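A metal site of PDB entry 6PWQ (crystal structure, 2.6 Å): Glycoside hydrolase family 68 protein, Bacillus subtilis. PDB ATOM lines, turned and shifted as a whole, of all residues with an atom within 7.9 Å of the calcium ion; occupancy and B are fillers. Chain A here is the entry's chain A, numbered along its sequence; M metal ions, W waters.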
ATOM      1  N   GLN A 197       9.606 -28.651 -22.893  1.00  0.00           N
ATOM      2  CA  GLN A 197       8.627 -29.395 -23.680  1.00  0.00           C
ATOM      3  C   GLN A 197       9.305 -29.962 -24.928  1.00  0.00           C
ATOM      4  O   GLN A 197      10.210 -29.344 -25.501  1.00  0.00           O
ATOM      5  CB  GLN A 197       7.466 -28.472 -24.059  1.00  0.00           C
ATOM      6  CG  GLN A 197       6.154 -29.182 -24.391  1.00  0.00           C
ATOM      7  CD  GLN A 197       5.093 -28.254 -24.980  1.00  0.00           C
ATOM      8  OE1 GLN A 197       5.344 -27.528 -25.947  1.00  0.00           O
ATOM      9  NE2 GLN A 197       3.888 -28.281 -24.391  1.00  0.00           N
ATOM     10  N   PHE A 202       3.729 -32.414 -27.435  1.00  0.00           N
ATOM     11  CA  PHE A 202       2.866 -31.688 -28.355  1.00  0.00           C
ATOM     12  C   PHE A 202       1.954 -32.636 -29.109  1.00  0.00           C
ATOM     13  O   PHE A 202       0.739 -32.407 -29.221  1.00  0.00           O
ATOM     14  CB  PHE A 202       3.740 -30.875 -29.318  1.00  0.00           C
ATOM     15  CG  PHE A 202       2.972 -30.079 -30.331  1.00  0.00           C
ATOM     16  CD1 PHE A 202       2.065 -29.110 -29.937  1.00  0.00           C
ATOM     17  CD2 PHE A 202       3.179 -30.286 -31.689  1.00  0.00           C
ATOM     18  CE1 PHE A 202       1.364 -28.376 -30.879  1.00  0.00           C
ATOM     19  CE2 PHE A 202       2.485 -29.558 -32.630  1.00  0.00           C
ATOM     20  CZ  PHE A 202       1.580 -28.601 -32.228  1.00  0.00           C
ATOM     21  N   GLU A 205      -0.897 -34.243 -26.963  1.00  0.00           N
ATOM     22  CA  GLU A 205      -1.989 -33.366 -26.536  1.00  0.00           C
ATOM     23  C   GLU A 205      -2.925 -32.994 -27.674  1.00  0.00           C
ATOM     24  O   GLU A 205      -3.847 -32.204 -27.462  1.00  0.00           O
ATOM     25  CB  GLU A 205      -1.452 -32.077 -25.914  1.00  0.00           C
ATOM     26  CG  GLU A 205      -0.883 -31.101 -26.930  1.00  0.00           C
ATOM     27  CD  GLU A 205      -0.234 -29.895 -26.287  1.00  0.00           C
ATOM     28  OE1 GLU A 205       0.804 -29.455 -26.828  1.00  0.00           O
ATOM     29  OE2 GLU A 205      -0.757 -29.373 -25.265  1.00  0.00           O
ATOM     30  N   GLY A 211      -4.461 -25.935 -29.768  1.00  0.00           N
ATOM     31  CA  GLY A 211      -4.131 -24.550 -29.516  1.00  0.00           C
ATOM     32  C   GLY A 211      -2.792 -24.324 -28.850  1.00  0.00           C
ATOM     33  O   GLY A 211      -2.439 -23.168 -28.593  1.00  0.00           O
ATOM     34  N   ASP A 212      -2.023 -25.386 -28.568  1.00  0.00           N
ATOM     35  CA  ASP A 212      -0.710 -25.190 -27.976  1.00  0.00           C
ATOM     36  C   ASP A 212       0.297 -24.777 -29.034  1.00  0.00           C
ATOM     37  O   ASP A 212       0.109 -24.997 -30.243  1.00  0.00           O
ATOM     38  CB  ASP A 212      -0.226 -26.460 -27.279  1.00  0.00           C
ATOM     39  CG  ASP A 212       0.802 -26.182 -26.186  1.00  0.00           C
ATOM     40  OD1 ASP A 212       0.845 -25.033 -25.703  1.00  0.00           O
ATOM     41  OD2 ASP A 212       1.547 -27.094 -25.790  1.00  0.00           O
ATOM     42  N   ASN A 213       1.400 -24.179 -28.571  1.00  0.00           N
ATOM     43  CA  ASN A 213       2.416 -23.592 -29.427  1.00  0.00           C
ATOM     44  C   ASN A 213       3.757 -24.148 -28.966  1.00  0.00           C
ATOM     45  O   ASN A 213       4.375 -23.609 -28.047  1.00  0.00           O
ATOM     46  CB  ASN A 213       2.371 -22.073 -29.350  1.00  0.00           C
ATOM     47  CG  ASN A 213       3.192 -21.387 -30.418  1.00  0.00           C
ATOM     48  OD1 ASN A 213       3.999 -22.017 -31.101  1.00  0.00           O
ATOM     49  ND2 ASN A 213       3.004 -20.074 -30.557  1.00  0.00           N
ATOM     50  N   HIS A 214       4.212 -25.244 -29.588  1.00  0.00           N
ATOM     51  CA  HIS A 214       5.442 -25.899 -29.156  1.00  0.00           C
ATOM     52  C   HIS A 214       6.635 -25.259 -29.842  1.00  0.00           C
ATOM     53  O   HIS A 214       6.721 -25.258 -31.083  1.00  0.00           O
ATOM     54  CB  HIS A 214       5.422 -27.389 -29.459  1.00  0.00           C
ATOM     55  CG  HIS A 214       6.762 -28.027 -29.292  1.00  0.00           C
ATOM     56  ND1 HIS A 214       7.347 -28.222 -28.056  1.00  0.00           N
ATOM     57  CD2 HIS A 214       7.664 -28.467 -30.206  1.00  0.00           C
ATOM     58  CE1 HIS A 214       8.537 -28.779 -28.208  1.00  0.00           C
ATOM     59  NE2 HIS A 214       8.754 -28.931 -29.506  1.00  0.00           N
ATOM     60  N   THR A 215       7.565 -24.737 -29.060  1.00  0.00           N
ATOM     61  CA  THR A 215       8.744 -24.081 -29.600  1.00  0.00           C
ATOM     62  C   THR A 215       9.987 -24.698 -28.997  1.00  0.00           C
ATOM     63  O   THR A 215       9.976 -25.181 -27.853  1.00  0.00           O
ATOM     64  CB  THR A 215       8.727 -22.547 -29.326  1.00  0.00           C
ATOM     65  OG1 THR A 215       9.072 -22.303 -27.970  1.00  0.00           O
ATOM     66  CG2 THR A 215       7.352 -21.948 -29.624  1.00  0.00           C
ATOM     67  N   ALA A 234      12.103 -21.823 -25.751  1.00  0.00           N
ATOM     68  CA  ALA A 234      11.521 -23.136 -25.512  1.00  0.00           C
ATOM     69  C   ALA A 234      10.215 -22.965 -24.752  1.00  0.00           C
ATOM     70  O   ALA A 234       9.669 -21.861 -24.657  1.00  0.00           O
ATOM     71  CB  ALA A 234      12.499 -24.025 -24.744  1.00  0.00           C
ATOM     72  N   ASN A 235       9.712 -24.065 -24.211  1.00  0.00           N
ATOM     73  CA  ASN A 235       8.574 -24.069 -23.315  1.00  0.00           C
ATOM     74  C   ASN A 235       8.918 -24.912 -22.097  1.00  0.00           C
ATOM     75  O   ASN A 235       9.757 -25.823 -22.168  1.00  0.00           O
ATOM     76  CB  ASN A 235       7.349 -24.615 -24.020  1.00  0.00           C
ATOM     77  CG  ASN A 235       6.902 -23.731 -25.147  1.00  0.00           C
ATOM     78  OD1 ASN A 235       7.346 -23.884 -26.286  1.00  0.00           O
ATOM     79  ND2 ASN A 235       6.021 -22.782 -24.835  1.00  0.00           N
ATOM     80  N   THR A 236       8.277 -24.602 -20.967  1.00  0.00           N
ATOM     81  CA  THR A 236       8.591 -25.323 -19.734  1.00  0.00           C
ATOM     82  C   THR A 236       8.114 -26.762 -19.836  1.00  0.00           C
ATOM     83  O   THR A 236       7.180 -27.083 -20.570  1.00  0.00           O
ATOM     84  CB  THR A 236       7.943 -24.657 -18.525  1.00  0.00           C
ATOM     85  OG1 THR A 236       6.514 -24.690 -18.688  1.00  0.00           O
ATOM     86  CG2 THR A 236       8.415 -23.225 -18.359  1.00  0.00           C
ATOM     87  N   TYR A 242       4.722 -26.308 -15.551  1.00  0.00           N
ATOM     88  CA  TYR A 242       4.128 -26.703 -16.821  1.00  0.00           C
ATOM     89  C   TYR A 242       2.813 -25.979 -17.056  1.00  0.00           C
ATOM     90  O   TYR A 242       2.230 -25.369 -16.156  1.00  0.00           O
ATOM     91  CB  TYR A 242       3.908 -28.213 -16.892  1.00  0.00           C
ATOM     92  CG  TYR A 242       3.765 -28.730 -18.315  1.00  0.00           C
ATOM     93  CD1 TYR A 242       4.763 -28.513 -19.253  1.00  0.00           C
ATOM     94  CD2 TYR A 242       2.644 -29.438 -18.708  1.00  0.00           C
ATOM     95  CE1 TYR A 242       4.655 -28.981 -20.554  1.00  0.00           C
ATOM     96  CE2 TYR A 242       2.519 -29.910 -20.011  1.00  0.00           C
ATOM     97  CZ  TYR A 242       3.528 -29.675 -20.927  1.00  0.00           C
ATOM     98  OH  TYR A 242       3.416 -30.131 -22.223  1.00  0.00           O
ATOM     99  N   GLN A 243       2.350 -26.045 -18.313  1.00  0.00           N
ATOM    100  CA  GLN A 243       1.067 -25.487 -18.709  1.00  0.00           C
ATOM    101  C   GLN A 243      -0.077 -26.256 -18.042  1.00  0.00           C
ATOM    102  O   GLN A 243       0.133 -27.252 -17.323  1.00  0.00           O
ATOM    103  CB  GLN A 243       0.927 -25.509 -20.228  1.00  0.00           C
ATOM    104  CG  GLN A 243       1.007 -26.906 -20.811  1.00  0.00           C
ATOM    105  CD  GLN A 243       1.293 -26.903 -22.297  1.00  0.00           C
ATOM    106  OE1 GLN A 243       1.994 -26.029 -22.802  1.00  0.00           O
ATOM    107  NE2 GLN A 243       0.753 -27.900 -23.014  1.00  0.00           N
ATOM    108  N   GLY A 244      -1.296 -25.799 -18.265  1.00  0.00           N
ATOM    109  CA  GLY A 244      -2.482 -26.412 -17.700  1.00  0.00           C
ATOM    110  C   GLY A 244      -3.301 -25.435 -16.888  1.00  0.00           C
ATOM    111  O   GLY A 244      -2.879 -24.325 -16.561  1.00  0.00           O
ATOM    112  N   THR A 276      -5.895 -19.501 -23.625  1.00  0.00           N
ATOM    113  CA  THR A 276      -4.569 -19.121 -24.103  1.00  0.00           C
ATOM    114  C   THR A 276      -3.582 -18.980 -22.948  1.00  0.00           C
ATOM    115  O   THR A 276      -2.415 -19.346 -23.075  1.00  0.00           O
ATOM    116  CB  THR A 276      -4.650 -17.819 -24.900  1.00  0.00           C
ATOM    117  OG1 THR A 276      -5.622 -17.950 -25.947  1.00  0.00           O
ATOM    118  CG2 THR A 276      -3.297 -17.487 -25.522  1.00  0.00           C
ATOM    119  N   ALA A 277      -4.050 -18.463 -21.812  1.00  0.00           N
ATOM    120  CA  ALA A 277      -3.173 -18.337 -20.656  1.00  0.00           C
ATOM    121  C   ALA A 277      -2.787 -19.703 -20.107  1.00  0.00           C
ATOM    122  O   ALA A 277      -1.623 -19.916 -19.731  1.00  0.00           O
ATOM    123  CB  ALA A 277      -3.847 -17.501 -19.570  1.00  0.00           C
ATOM    124  N   GLU A 278      -3.726 -20.659 -20.078  1.00  0.00           N
ATOM    125  CA  GLU A 278      -3.426 -21.966 -19.516  1.00  0.00           C
ATOM    126  C   GLU A 278      -2.362 -22.688 -20.330  1.00  0.00           C
ATOM    127  O   GLU A 278      -1.565 -23.445 -19.768  1.00  0.00           O
ATOM    128  CB  GLU A 278      -4.684 -22.809 -19.423  1.00  0.00           C
ATOM    129  CG  GLU A 278      -5.646 -22.351 -18.339  1.00  0.00           C
ATOM    130  CD  GLU A 278      -6.999 -23.054 -18.434  1.00  0.00           C
ATOM    131  OE1 GLU A 278      -7.192 -23.850 -19.371  1.00  0.00           O
ATOM    132  OE2 GLU A 278      -7.854 -22.797 -17.564  1.00  0.00           O
ATOM    133  N   LEU A 279      -2.306 -22.448 -21.636  1.00  0.00           N
ATOM    134  CA  LEU A 279      -1.328 -23.081 -22.504  1.00  0.00           C
ATOM    135  C   LEU A 279      -0.035 -22.268 -22.633  1.00  0.00           C
ATOM    136  O   LEU A 279       0.976 -22.794 -23.119  1.00  0.00           O
ATOM    137  CB  LEU A 279      -1.942 -23.311 -23.882  1.00  0.00           C
ATOM    138  CG  LEU A 279      -3.005 -24.394 -23.809  1.00  0.00           C
ATOM    139  CD1 LEU A 279      -3.739 -24.565 -25.144  1.00  0.00           C
ATOM    140  CD2 LEU A 279      -2.345 -25.678 -23.374  1.00  0.00           C
ATOM    141  N   ALA A 280      -0.039 -21.000 -22.194  1.00  0.00           N
ATOM    142  CA  ALA A 280       1.127 -20.141 -22.294  1.00  0.00           C
ATOM    143  C   ALA A 280       2.188 -20.564 -21.265  1.00  0.00           C
ATOM    144  O   ALA A 280       2.012 -20.341 -20.060  1.00  0.00           O
ATOM    145  CB  ALA A 280       0.719 -18.691 -22.079  1.00  0.00           C
ATOM    146  N   ASN A 281       3.289 -21.152 -21.734  1.00  0.00           N
ATOM    147  CA  ASN A 281       4.419 -21.459 -20.862  1.00  0.00           C
ATOM    148  C   ASN A 281       5.739 -21.282 -21.618  1.00  0.00           C
ATOM    149  O   ASN A 281       6.631 -22.141 -21.579  1.00  0.00           O
ATOM    150  CB  ASN A 281       4.293 -22.871 -20.283  1.00  0.00           C
ATOM    151  CG  ASN A 281       4.403 -23.952 -21.359  1.00  0.00           C
ATOM    152  OD1 ASN A 281       3.916 -23.774 -22.481  1.00  0.00           O
ATOM    153  ND2 ASN A 281       5.063 -25.062 -21.023  1.00  0.00           N
ATOM    154  N   GLY A 282       5.899 -20.154 -22.291  1.00  0.00           N
ATOM    155  CA  GLY A 282       7.167 -19.877 -22.948  1.00  0.00           C
ATOM    156  C   GLY A 282       8.310 -19.811 -21.953  1.00  0.00           C
ATOM    157  O   GLY A 282       8.125 -19.542 -20.767  1.00  0.00           O
ATOM    158  N   THR A 309       2.640 -15.637 -22.234  1.00  0.00           N
ATOM    159  CA  THR A 309       2.696 -16.020 -23.635  1.00  0.00           C
ATOM    160  C   THR A 309       3.392 -17.361 -23.770  1.00  0.00           C
ATOM    161  O   THR A 309       4.165 -17.776 -22.901  1.00  0.00           O
ATOM    162  CB  THR A 309       3.422 -14.973 -24.500  1.00  0.00           C
ATOM    163  OG1 THR A 309       3.468 -15.434 -25.860  1.00  0.00           O
ATOM    164  CG2 THR A 309       4.835 -14.742 -23.976  1.00  0.00           C
ATOM    165  N   ASP A 310       3.097 -18.039 -24.887  1.00  0.00           N
ATOM    166  CA  ASP A 310       3.760 -19.285 -25.248  1.00  0.00           C
ATOM    167  C   ASP A 310       4.979 -19.068 -26.135  1.00  0.00           C
ATOM    168  O   ASP A 310       5.709 -20.026 -26.417  1.00  0.00           O
ATOM    169  CB  ASP A 310       2.766 -20.197 -25.973  1.00  0.00           C
ATOM    170  CG  ASP A 310       2.749 -21.630 -25.422  1.00  0.00           C
ATOM    171  OD1 ASP A 310       3.443 -21.904 -24.402  1.00  0.00           O
ATOM    172  OD2 ASP A 310       2.013 -22.467 -25.998  1.00  0.00           O
ATOM    173  N   GLU A 311       5.249 -17.839 -26.559  1.00  0.00           N
ATOM    174  CA  GLU A 311       6.196 -17.619 -27.639  1.00  0.00           C
ATOM    175  C   GLU A 311       7.062 -16.405 -27.297  1.00  0.00           C
ATOM    176  O   GLU A 311       6.639 -15.257 -27.484  1.00  0.00           O
ATOM    177  CB  GLU A 311       5.449 -17.409 -28.954  1.00  0.00           C
ATOM    178  CG  GLU A 311       6.336 -17.481 -30.170  1.00  0.00           C
ATOM    179  CD  GLU A 311       5.557 -17.329 -31.450  1.00  0.00           C
ATOM    180  OE1 GLU A 311       4.981 -18.342 -31.926  1.00  0.00           O
ATOM    181  OE2 GLU A 311       5.499 -16.200 -31.980  1.00  0.00           O
HETATM  182 CA    CA M   1       2.553 -24.275 -24.272  1.00  0.00          CA
HETATM  183  O   HOH W   1       4.251 -25.124 -25.902  1.00  0.00           O
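The side-chain carboxylate (OE1) of Glu 205 sits close to the side-chain carboxylate (OD2) of Asp 212, 2.7 Å away. The backbone carbonyl oxygen (O) of Asn 281 lies close to the side-chain amide nitrogen (ND2) of Asn 235. OD2 of Asp 212 sits at hydrogen-bond distance from NE2 of Gln 197 (3.0 Å). The side-chain amide nitrogen (NE2) of Gln 243 sits close to the side-chain amide nitrogen (NE2) of Gln 197 (3.4 Å). The side-chain amide nitrogen of Asn 235 is in hydrogen-bond range of the backbone carbonyl oxygen of Asp 310 (3.2 Å). N of Asn 213 lies close to OD2 of Asp 310, 3.2 Å away. The side-chain amide oxygen (OD1) of Asn 235 sits close to the backbone carbonyl oxygen (O) of Asn 213. OD1 of Asn 235 lies within hydrogen-bond range of OG1 of Thr 215 (2.9 Å).
Merely in contact with the calcium ion: Asn 235 (3.8 Å). Of the 24 residues printed, 6 come within 4 Å of the calcium ion. The nearest printed residue that does not touch the calcium ion is Gln 197 (4.2 Å).
The calcium ion is bound by the side-chain amide oxygen (OD1) of Asn 281, 2.3 Å away. OD1 of Asp 212 is bound to the calcium ion, at 2.4 Å. OE1 of Gln 243 binds the calcium ion, 2.4 Å away. The backbone carbonyl oxygen (O) of Leu 279 binds the calcium ion, 2.5 Å away. The calcium ion is bound by water W1 (2.5 Å). The side-chain carboxylate (OD1) of Asp 310 is bound to the calcium ion, 2.5 Å away. The side-chain carboxylate (OD2) of Asp 310 binds the calcium ion, 2.6 Å away. The calcium ion has seven donor atoms within binding distance.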
